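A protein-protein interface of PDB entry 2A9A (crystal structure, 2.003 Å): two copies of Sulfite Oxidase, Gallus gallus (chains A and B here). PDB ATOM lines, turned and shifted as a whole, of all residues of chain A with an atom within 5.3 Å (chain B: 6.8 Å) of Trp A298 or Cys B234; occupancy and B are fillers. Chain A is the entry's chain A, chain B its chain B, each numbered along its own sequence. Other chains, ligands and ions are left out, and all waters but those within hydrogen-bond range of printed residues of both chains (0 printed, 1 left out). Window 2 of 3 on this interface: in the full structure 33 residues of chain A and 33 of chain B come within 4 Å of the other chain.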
ATOM      1  N   ASP A 289      14.668 -25.226  31.082  1.00  0.00           N
ATOM      2  CA  ASP A 289      14.676 -24.937  29.639  1.00  0.00           C
ATOM      3  C   ASP A 289      15.852 -25.634  28.985  1.00  0.00           C
ATOM      4  O   ASP A 289      16.945 -25.588  29.530  1.00  0.00           O
ATOM      5  CB  ASP A 289      14.804 -23.439  29.393  1.00  0.00           C
ATOM      6  CG  ASP A 289      13.641 -22.660  29.927  1.00  0.00           C
ATOM      7  OD1 ASP A 289      12.534 -23.262  29.974  1.00  0.00           O
ATOM      8  OD2 ASP A 289      13.834 -21.431  30.205  1.00  0.00           O
ATOM      9  N   VAL A 290      15.611 -26.284  27.831  1.00  0.00           N
ATOM     10  CA  VAL A 290      16.650 -27.000  27.078  1.00  0.00           C
ATOM     11  C   VAL A 290      16.698 -26.535  25.606  1.00  0.00           C
ATOM     12  O   VAL A 290      15.661 -26.340  25.001  1.00  0.00           O
ATOM     13  CB  VAL A 290      16.426 -28.525  27.107  1.00  0.00           C
ATOM     14  CG1 VAL A 290      17.544 -29.249  26.388  1.00  0.00           C
ATOM     15  CG2 VAL A 290      16.364 -28.984  28.495  1.00  0.00           C
ATOM     16  N   SER A 291      17.894 -26.232  25.109  1.00  0.00           N
ATOM     17  CA  SER A 291      18.091 -25.799  23.749  1.00  0.00           C
ATOM     18  C   SER A 291      18.932 -26.831  23.022  1.00  0.00           C
ATOM     19  O   SER A 291      19.735 -27.505  23.662  1.00  0.00           O
ATOM     20  CB  SER A 291      18.820 -24.470  23.738  1.00  0.00           C
ATOM     21  OG  SER A 291      19.025 -24.023  22.434  1.00  0.00           O
ATOM     22  N   GLY A 295      21.238 -22.171  22.548  1.00  0.00           N
ATOM     23  CA  GLY A 295      20.553 -21.145  23.323  1.00  0.00           C
ATOM     24  C   GLY A 295      19.750 -20.128  22.532  1.00  0.00           C
ATOM     25  O   GLY A 295      19.324 -19.113  23.085  1.00  0.00           O
ATOM     26  N   ARG A 296      19.550 -20.378  21.248  1.00  0.00           N
ATOM     27  CA  ARG A 296      18.759 -19.484  20.451  1.00  0.00           C
ATOM     28  C   ARG A 296      17.285 -19.805  20.680  1.00  0.00           C
ATOM     29  O   ARG A 296      16.464 -18.893  20.807  1.00  0.00           O
ATOM     30  CB  ARG A 296      19.117 -19.631  19.005  1.00  0.00           C
ATOM     31  CG  ARG A 296      20.550 -19.334  18.736  1.00  0.00           C
ATOM     32  CD  ARG A 296      20.748 -19.037  17.289  1.00  0.00           C
ATOM     33  NE  ARG A 296      21.991 -19.608  16.834  1.00  0.00           N
ATOM     34  CZ  ARG A 296      22.087 -20.701  16.091  1.00  0.00           C
ATOM     35  NH1 ARG A 296      21.007 -21.283  15.559  1.00  0.00           N
ATOM     36  NH2 ARG A 296      23.295 -21.179  15.825  1.00  0.00           N
ATOM     37  N   THR A 297      16.931 -21.089  20.641  1.00  0.00           N
ATOM     38  CA  THR A 297      15.556 -21.492  20.949  1.00  0.00           C
ATOM     39  C   THR A 297      15.540 -22.531  22.074  1.00  0.00           C
ATOM     40  O   THR A 297      16.506 -23.297  22.255  1.00  0.00           O
ATOM     41  CB  THR A 297      14.796 -22.003  19.716  1.00  0.00           C
ATOM     42  OG1 THR A 297      15.445 -23.158  19.188  1.00  0.00           O
ATOM     43  CG2 THR A 297      14.722 -20.904  18.642  1.00  0.00           C
ATOM     44  N   TRP A 298      14.413 -22.607  22.755  1.00  0.00           N
ATOM     45  CA  TRP A 298      14.249 -23.459  23.920  1.00  0.00           C
ATOM     46  C   TRP A 298      13.005 -24.317  23.922  1.00  0.00           C
ATOM     47  O   TRP A 298      11.996 -23.959  23.327  1.00  0.00           O
ATOM     48  CB  TRP A 298      14.199 -22.566  25.154  1.00  0.00           C
ATOM     49  CG  TRP A 298      15.372 -21.614  25.292  1.00  0.00           C
ATOM     50  CD1 TRP A 298      15.467 -20.349  24.760  1.00  0.00           C
ATOM     51  CD2 TRP A 298      16.630 -21.875  25.936  1.00  0.00           C
ATOM     52  NE1 TRP A 298      16.687 -19.792  25.093  1.00  0.00           N
ATOM     53  CE2 TRP A 298      17.433 -20.720  25.778  1.00  0.00           C
ATOM     54  CE3 TRP A 298      17.151 -22.955  26.645  1.00  0.00           C
ATOM     55  CZ2 TRP A 298      18.734 -20.622  26.318  1.00  0.00           C
ATOM     56  CZ3 TRP A 298      18.449 -22.869  27.156  1.00  0.00           C
ATOM     57  CH2 TRP A 298      19.212 -21.699  27.019  1.00  0.00           C
ATOM     58  N   LYS A 299      13.086 -25.433  24.642  1.00  0.00           N
ATOM     59  CA  LYS A 299      11.977 -26.368  24.878  1.00  0.00           C
ATOM     60  C   LYS A 299      11.971 -26.665  26.358  1.00  0.00           C
ATOM     61  O   LYS A 299      12.992 -26.449  27.030  1.00  0.00           O
ATOM     62  CB  LYS A 299      12.134 -27.636  24.042  1.00  0.00           C
ATOM     63  CG  LYS A 299      11.911 -27.354  22.537  1.00  0.00           C
ATOM     64  CD  LYS A 299      12.135 -28.615  21.648  1.00  0.00           C
ATOM     65  CE  LYS A 299      11.933 -28.327  20.125  1.00  0.00           C
ATOM     66  NZ  LYS A 299      10.591 -27.657  19.865  1.00  0.00           N
ATOM     67  N   VAL A 300      10.803 -27.002  26.894  1.00  0.00           N
ATOM     68  CA  VAL A 300      10.627 -27.277  28.316  1.00  0.00           C
ATOM     69  C   VAL A 300      10.788 -28.764  28.629  1.00  0.00           C
ATOM     70  O   VAL A 300      10.134 -29.610  28.025  1.00  0.00           O
ATOM     71  CB  VAL A 300       9.260 -26.753  28.804  1.00  0.00           C
ATOM     72  CG1 VAL A 300       9.001 -27.118  30.247  1.00  0.00           C
ATOM     73  CG2 VAL A 300       9.226 -25.229  28.659  1.00  0.00           C
ATOM     74  N   VAL A 334      22.097 -27.103  25.499  1.00  0.00           N
ATOM     75  CA  VAL A 334      22.269 -26.175  26.614  1.00  0.00           C
ATOM     76  C   VAL A 334      21.090 -26.334  27.537  1.00  0.00           C
ATOM     77  O   VAL A 334      19.996 -26.500  27.058  1.00  0.00           O
ATOM     78  CB  VAL A 334      22.291 -24.706  26.120  1.00  0.00           C
ATOM     79  CG1 VAL A 334      22.673 -23.752  27.252  1.00  0.00           C
ATOM     80  CG2 VAL A 334      23.259 -24.515  24.995  1.00  0.00           C
ATOM     81  N   CYS A 335      21.316 -26.299  28.855  1.00  0.00           N
ATOM     82  CA  CYS A 335      20.241 -26.319  29.870  1.00  0.00           C
ATOM     83  C   CYS A 335      20.338 -25.154  30.887  1.00  0.00           C
ATOM     84  O   CYS A 335      21.403 -24.587  31.163  1.00  0.00           O
ATOM     85  CB  CYS A 335      20.136 -27.676  30.617  1.00  0.00           C
ATOM     86  SG  CYS A 335      21.516 -28.135  31.660  1.00  0.00           S
ATOM     87  N   LYS A 336      19.169 -24.757  31.360  1.00  0.00           N
ATOM     88  CA  LYS A 336      19.067 -23.739  32.377  1.00  0.00           C
ATOM     89  C   LYS A 336      17.799 -23.980  33.184  1.00  0.00           C
ATOM     90  O   LYS A 336      16.750 -24.311  32.606  1.00  0.00           O
ATOM     91  CB  LYS A 336      19.155 -22.332  31.747  1.00  0.00           C
ATOM     92  CG  LYS A 336      17.998 -21.928  30.817  1.00  0.00           C
ATOM     93  CD  LYS A 336      18.295 -20.587  30.153  1.00  0.00           C
ATOM     94  CE  LYS A 336      17.179 -20.133  29.281  1.00  0.00           C
ATOM     95  NZ  LYS A 336      15.998 -19.553  29.955  1.00  0.00           N
ATOM     96  N   TRP A 363      25.259 -21.441  32.095  1.00  0.00           N
ATOM     97  CA  TRP A 363      24.649 -22.579  31.390  1.00  0.00           C
ATOM     98  C   TRP A 363      25.662 -23.596  30.927  1.00  0.00           C
ATOM     99  O   TRP A 363      26.709 -23.246  30.374  1.00  0.00           O
ATOM    100  CB  TRP A 363      23.831 -22.201  30.160  1.00  0.00           C
ATOM    101  CG  TRP A 363      22.949 -20.981  30.304  1.00  0.00           C
ATOM    102  CD1 TRP A 363      22.342 -20.553  31.409  1.00  0.00           C
ATOM    103  CD2 TRP A 363      22.517 -20.121  29.242  1.00  0.00           C
ATOM    104  NE1 TRP A 363      21.650 -19.396  31.138  1.00  0.00           N
ATOM    105  CE2 TRP A 363      21.716 -19.129  29.809  1.00  0.00           C
ATOM    106  CE3 TRP A 363      22.780 -20.069  27.885  1.00  0.00           C
ATOM    107  CZ2 TRP A 363      21.139 -18.097  29.062  1.00  0.00           C
ATOM    108  CZ3 TRP A 363      22.212 -19.034  27.129  1.00  0.00           C
ATOM    109  CH2 TRP A 363      21.419 -18.065  27.724  1.00  0.00           C
ATOM    110  N   ARG B 103      11.072  -8.435  22.001  1.00  0.00           N
ATOM    111  CA  ARG B 103       9.871  -8.751  21.250  1.00  0.00           C
ATOM    112  C   ARG B 103       8.682  -8.131  22.012  1.00  0.00           C
ATOM    113  O   ARG B 103       8.728  -7.993  23.232  1.00  0.00           O
ATOM    114  CB  ARG B 103       9.623 -10.255  21.084  1.00  0.00           C
ATOM    115  CG  ARG B 103      10.574 -10.967  20.222  1.00  0.00           C
ATOM    116  CD  ARG B 103      10.093 -12.383  19.844  1.00  0.00           C
ATOM    117  NE  ARG B 103      10.053 -13.345  20.950  1.00  0.00           N
ATOM    118  CZ  ARG B 103      11.129 -13.945  21.476  1.00  0.00           C
ATOM    119  NH1 ARG B 103      12.360 -13.566  21.125  1.00  0.00           N
ATOM    120  NH2 ARG B 103      10.979 -14.860  22.453  1.00  0.00           N
ATOM    121  N   PHE B 231       7.249 -17.837  32.358  1.00  0.00           N
ATOM    122  CA  PHE B 231       7.218 -18.878  31.345  1.00  0.00           C
ATOM    123  C   PHE B 231       8.505 -18.909  30.587  1.00  0.00           C
ATOM    124  O   PHE B 231       9.244 -17.922  30.570  1.00  0.00           O
ATOM    125  CB  PHE B 231       6.054 -18.632  30.355  1.00  0.00           C
ATOM    126  CG  PHE B 231       4.710 -18.654  31.018  1.00  0.00           C
ATOM    127  CD1 PHE B 231       4.146 -19.837  31.413  1.00  0.00           C
ATOM    128  CD2 PHE B 231       4.088 -17.490  31.380  1.00  0.00           C
ATOM    129  CE1 PHE B 231       2.931 -19.847  32.144  1.00  0.00           C
ATOM    130  CE2 PHE B 231       2.875 -17.498  32.070  1.00  0.00           C
ATOM    131  CZ  PHE B 231       2.322 -18.688  32.462  1.00  0.00           C
ATOM    132  N   SER B 232       8.751 -20.063  29.961  1.00  0.00           N
ATOM    133  CA  SER B 232       9.853 -20.281  29.060  1.00  0.00           C
ATOM    134  C   SER B 232       9.778 -19.228  27.939  1.00  0.00           C
ATOM    135  O   SER B 232       8.676 -18.867  27.512  1.00  0.00           O
ATOM    136  CB  SER B 232       9.701 -21.702  28.475  1.00  0.00           C
ATOM    137  OG  SER B 232      10.717 -22.001  27.555  1.00  0.00           O
ATOM    138  N   PRO B 233      10.921 -18.753  27.416  1.00  0.00           N
ATOM    139  CA  PRO B 233      10.839 -17.763  26.293  1.00  0.00           C
ATOM    140  C   PRO B 233      10.109 -18.254  25.030  1.00  0.00           C
ATOM    141  O   PRO B 233       9.718 -17.427  24.171  1.00  0.00           O
ATOM    142  CB  PRO B 233      12.308 -17.507  25.943  1.00  0.00           C
ATOM    143  CG  PRO B 233      13.065 -18.607  26.580  1.00  0.00           C
ATOM    144  CD  PRO B 233      12.315 -19.027  27.785  1.00  0.00           C
ATOM    145  N   CYS B 234       9.976 -19.575  24.897  1.00  0.00           N
ATOM    146  CA  CYS B 234       9.270 -20.201  23.788  1.00  0.00           C
ATOM    147  C   CYS B 234       7.721 -20.065  23.839  1.00  0.00           C
ATOM    148  O   CYS B 234       7.062 -20.196  22.818  1.00  0.00           O
ATOM    149  CB  CYS B 234       9.625 -21.704  23.698  1.00  0.00           C
ATOM    150  SG  CYS B 234       9.026 -22.819  25.070  1.00  0.00           S
ATOM    151  N   VAL B 235       7.163 -19.784  25.012  1.00  0.00           N
ATOM    152  CA  VAL B 235       5.728 -19.690  25.169  1.00  0.00           C
ATOM    153  C   VAL B 235       5.160 -18.446  24.512  1.00  0.00           C
ATOM    154  O   VAL B 235       5.744 -17.369  24.591  1.00  0.00           O
ATOM    155  CB  VAL B 235       5.300 -19.759  26.654  1.00  0.00           C
ATOM    156  CG1 VAL B 235       3.851 -19.425  26.795  1.00  0.00           C
ATOM    157  CG2 VAL B 235       5.598 -21.134  27.207  1.00  0.00           C
ATOM    158  N   ASP B 236       4.018 -18.612  23.854  1.00  0.00           N
ATOM    159  CA  ASP B 236       3.339 -17.499  23.237  1.00  0.00           C
ATOM    160  C   ASP B 236       1.839 -17.554  23.576  1.00  0.00           C
ATOM    161  O   ASP B 236       1.367 -18.492  24.173  1.00  0.00           O
ATOM    162  CB  ASP B 236       3.588 -17.510  21.721  1.00  0.00           C
ATOM    163  CG  ASP B 236       3.369 -16.119  21.086  1.00  0.00           C
ATOM    164  OD1 ASP B 236       3.157 -15.126  21.838  1.00  0.00           O
ATOM    165  OD2 ASP B 236       3.443 -16.027  19.849  1.00  0.00           O
ATOM    166  N   ASP B 238      -0.800 -18.342  22.066  1.00  0.00           N
ATOM    167  CA  ASP B 238      -1.540 -19.515  21.652  1.00  0.00           C
ATOM    168  C   ASP B 238      -1.177 -20.798  22.393  1.00  0.00           C
ATOM    169  O   ASP B 238      -1.904 -21.771  22.259  1.00  0.00           O
ATOM    170  CB  ASP B 238      -1.473 -19.724  20.143  1.00  0.00           C
ATOM    171  CG  ASP B 238      -0.064 -19.911  19.615  1.00  0.00           C
ATOM    172  OD1 ASP B 238       0.935 -19.826  20.361  1.00  0.00           O
ATOM    173  OD2 ASP B 238       0.047 -20.088  18.399  1.00  0.00           O
ATOM    174  N   THR B 239      -0.092 -20.798  23.181  1.00  0.00           N
ATOM    175  CA  THR B 239       0.301 -21.984  23.967  1.00  0.00           C
ATOM    176  C   THR B 239       0.436 -21.755  25.485  1.00  0.00           C
ATOM    177  O   THR B 239       0.578 -22.708  26.240  1.00  0.00           O
ATOM    178  CB  THR B 239       1.625 -22.589  23.443  1.00  0.00           C
ATOM    179  OG1 THR B 239       2.686 -21.634  23.557  1.00  0.00           O
ATOM    180  CG2 THR B 239       1.475 -23.010  21.975  1.00  0.00           C
ATOM    181  N   ALA B 350      17.002 -11.779  26.100  1.00  0.00           N
ATOM    182  CA  ALA B 350      16.276 -12.746  25.267  1.00  0.00           C
ATOM    183  C   ALA B 350      15.999 -14.116  25.926  1.00  0.00           C
ATOM    184  O   ALA B 350      14.853 -14.604  25.870  1.00  0.00           O
ATOM    185  CB  ALA B 350      16.944 -12.909  23.887  1.00  0.00           C
ATOM    186  N   PRO B 351      17.001 -14.716  26.603  1.00  0.00           N
ATOM    187  CA  PRO B 351      16.754 -16.001  27.224  1.00  0.00           C
ATOM    188  C   PRO B 351      15.803 -15.980  28.413  1.00  0.00           C
ATOM    189  O   PRO B 351      15.362 -17.060  28.791  1.00  0.00           O
ATOM    190  CB  PRO B 351      18.159 -16.472  27.654  1.00  0.00           C
ATOM    191  CG  PRO B 351      19.143 -15.648  26.829  1.00  0.00           C
ATOM    192  CD  PRO B 351      18.403 -14.302  26.816  1.00  0.00           C
ATOM    193  N   ILE B 352      15.520 -14.803  29.008  1.00  0.00           N
ATOM    194  CA  ILE B 352      14.507 -14.694  30.090  1.00  0.00           C
ATOM    195  C   ILE B 352      13.222 -14.019  29.575  1.00  0.00           C
ATOM    196  O   ILE B 352      12.379 -13.625  30.353  1.00  0.00           O
ATOM    197  CB  ILE B 352      15.006 -13.971  31.340  1.00  0.00           C
ATOM    198  CG1 ILE B 352      15.495 -12.546  31.043  1.00  0.00           C
ATOM    199  CG2 ILE B 352      16.112 -14.769  32.005  1.00  0.00           C
ATOM    200  CD1 ILE B 352      15.623 -11.668  32.250  1.00  0.00           C
ATOM    201  N   TRP B 353      13.085 -13.906  28.255  1.00  0.00           N
ATOM    202  CA  TRP B 353      11.935 -13.273  27.706  1.00  0.00           C
ATOM    203  C   TRP B 353      10.691 -14.090  28.023  1.00  0.00           C
ATOM    204  O   TRP B 353      10.764 -15.307  28.223  1.00  0.00           O
ATOM    205  CB  TRP B 353      12.089 -13.080  26.203  1.00  0.00           C
ATOM    206  CG  TRP B 353      11.007 -12.265  25.556  1.00  0.00           C
ATOM    207  CD1 TRP B 353      10.984 -10.888  25.368  1.00  0.00           C
ATOM    208  CD2 TRP B 353       9.744 -12.745  25.075  1.00  0.00           C
ATOM    209  NE1 TRP B 353       9.796 -10.511  24.774  1.00  0.00           N
ATOM    210  CE2 TRP B 353       9.029 -11.624  24.567  1.00  0.00           C
ATOM    211  CE3 TRP B 353       9.175 -14.023  24.963  1.00  0.00           C
ATOM    212  CZ2 TRP B 353       7.778 -11.740  23.990  1.00  0.00           C
ATOM    213  CZ3 TRP B 353       7.905 -14.133  24.399  1.00  0.00           C
ATOM    214  CH2 TRP B 353       7.229 -12.997  23.913  1.00  0.00           C
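O of Pro B233 sits at hydrogen-bond distance from NH2 of Arg B103, 3.3 Å away. The side-chain carboxylate (OD2) of Asp A289 is in salt-bridge range of the side-chain amino group (NZ) of Lys A336, at 2.9 Å. The indole nitrogen of Trp A298 sits at hydrogen-bond distance from the backbone carbonyl oxygen of Gly A295, at 3.4 Å. OG of Ser B232 lies within hydrogen-bond range of SG of Cys B234, at 3.1 Å.
The side-chain sulfur (SG) of Cys B234 sits close to the backbone carbonyl oxygen (O) of Trp A298 (3.6 Å). The side-chain carboxylate of Asp A289 sits at hydrogen-bond distance from the side-chain hydroxyl of Ser B232. NZ of Lys A336 lies within hydrogen-bond range of O of Pro B351, 2.8 Å away.
No position is printed for both chains. Of the 7 pairs that touch across the chains among the printed residues, none has its exchanged pair printed and touching as well.
Printed residues of chain B within 4 Å of Asp A289: Ser B232 and Pro B233. Of the printed residues of chain B, Trp A298 touches Pro B233 and Cys B234. Of the printed residues of chain B, Val A300 touches Ser B232 (3.6 Å). Of the printed residues of chain B, Lys A336 touches Pro B351 (2.8 Å). Of the printed residues of chain B, Trp A363 touches Pro B351 (3.4 Å). Cys B234 touches one residue of chain A. Of the printed residues of chain A, Pro B351 touches Lys A336 (2.8 Å) and Trp A363 (3.4 Å). The nearest residue of chain A that does not touch Cys B234 is Val A300 (4.3 Å). The nearest printed residue of chain B that does not touch Lys A336 is Pro B233 (4.3 Å).
Printed residues of chain A that touch a printed residue of chain B: Asp A289, Trp A298, Val A300, Lys A336 and Trp A363. Hydrophobic or aromatic side chains of chain A that line the printed part of chain B: Trp A298, Val A300 and Trp A363. Of the 13 printed residues of chain B, 4 touch a printed residue of chain A. Hydrophobic or aromatic side chains of chain B that line the printed part of chain A: Pro B233 and Pro B351. Among the printed residues, 7 pairs touch across the chains. Among the printed residues, no Asp or Glu carboxylate lies within 4 Å of a Lys or Arg side-chain nitrogen of the other chain.
Among the printed residues, merely in contact across the chains: Trp A363 with Pro B351, Trp A298 with Pro B233, Val A300 with Ser B232 and Asp A289 with Pro B233.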
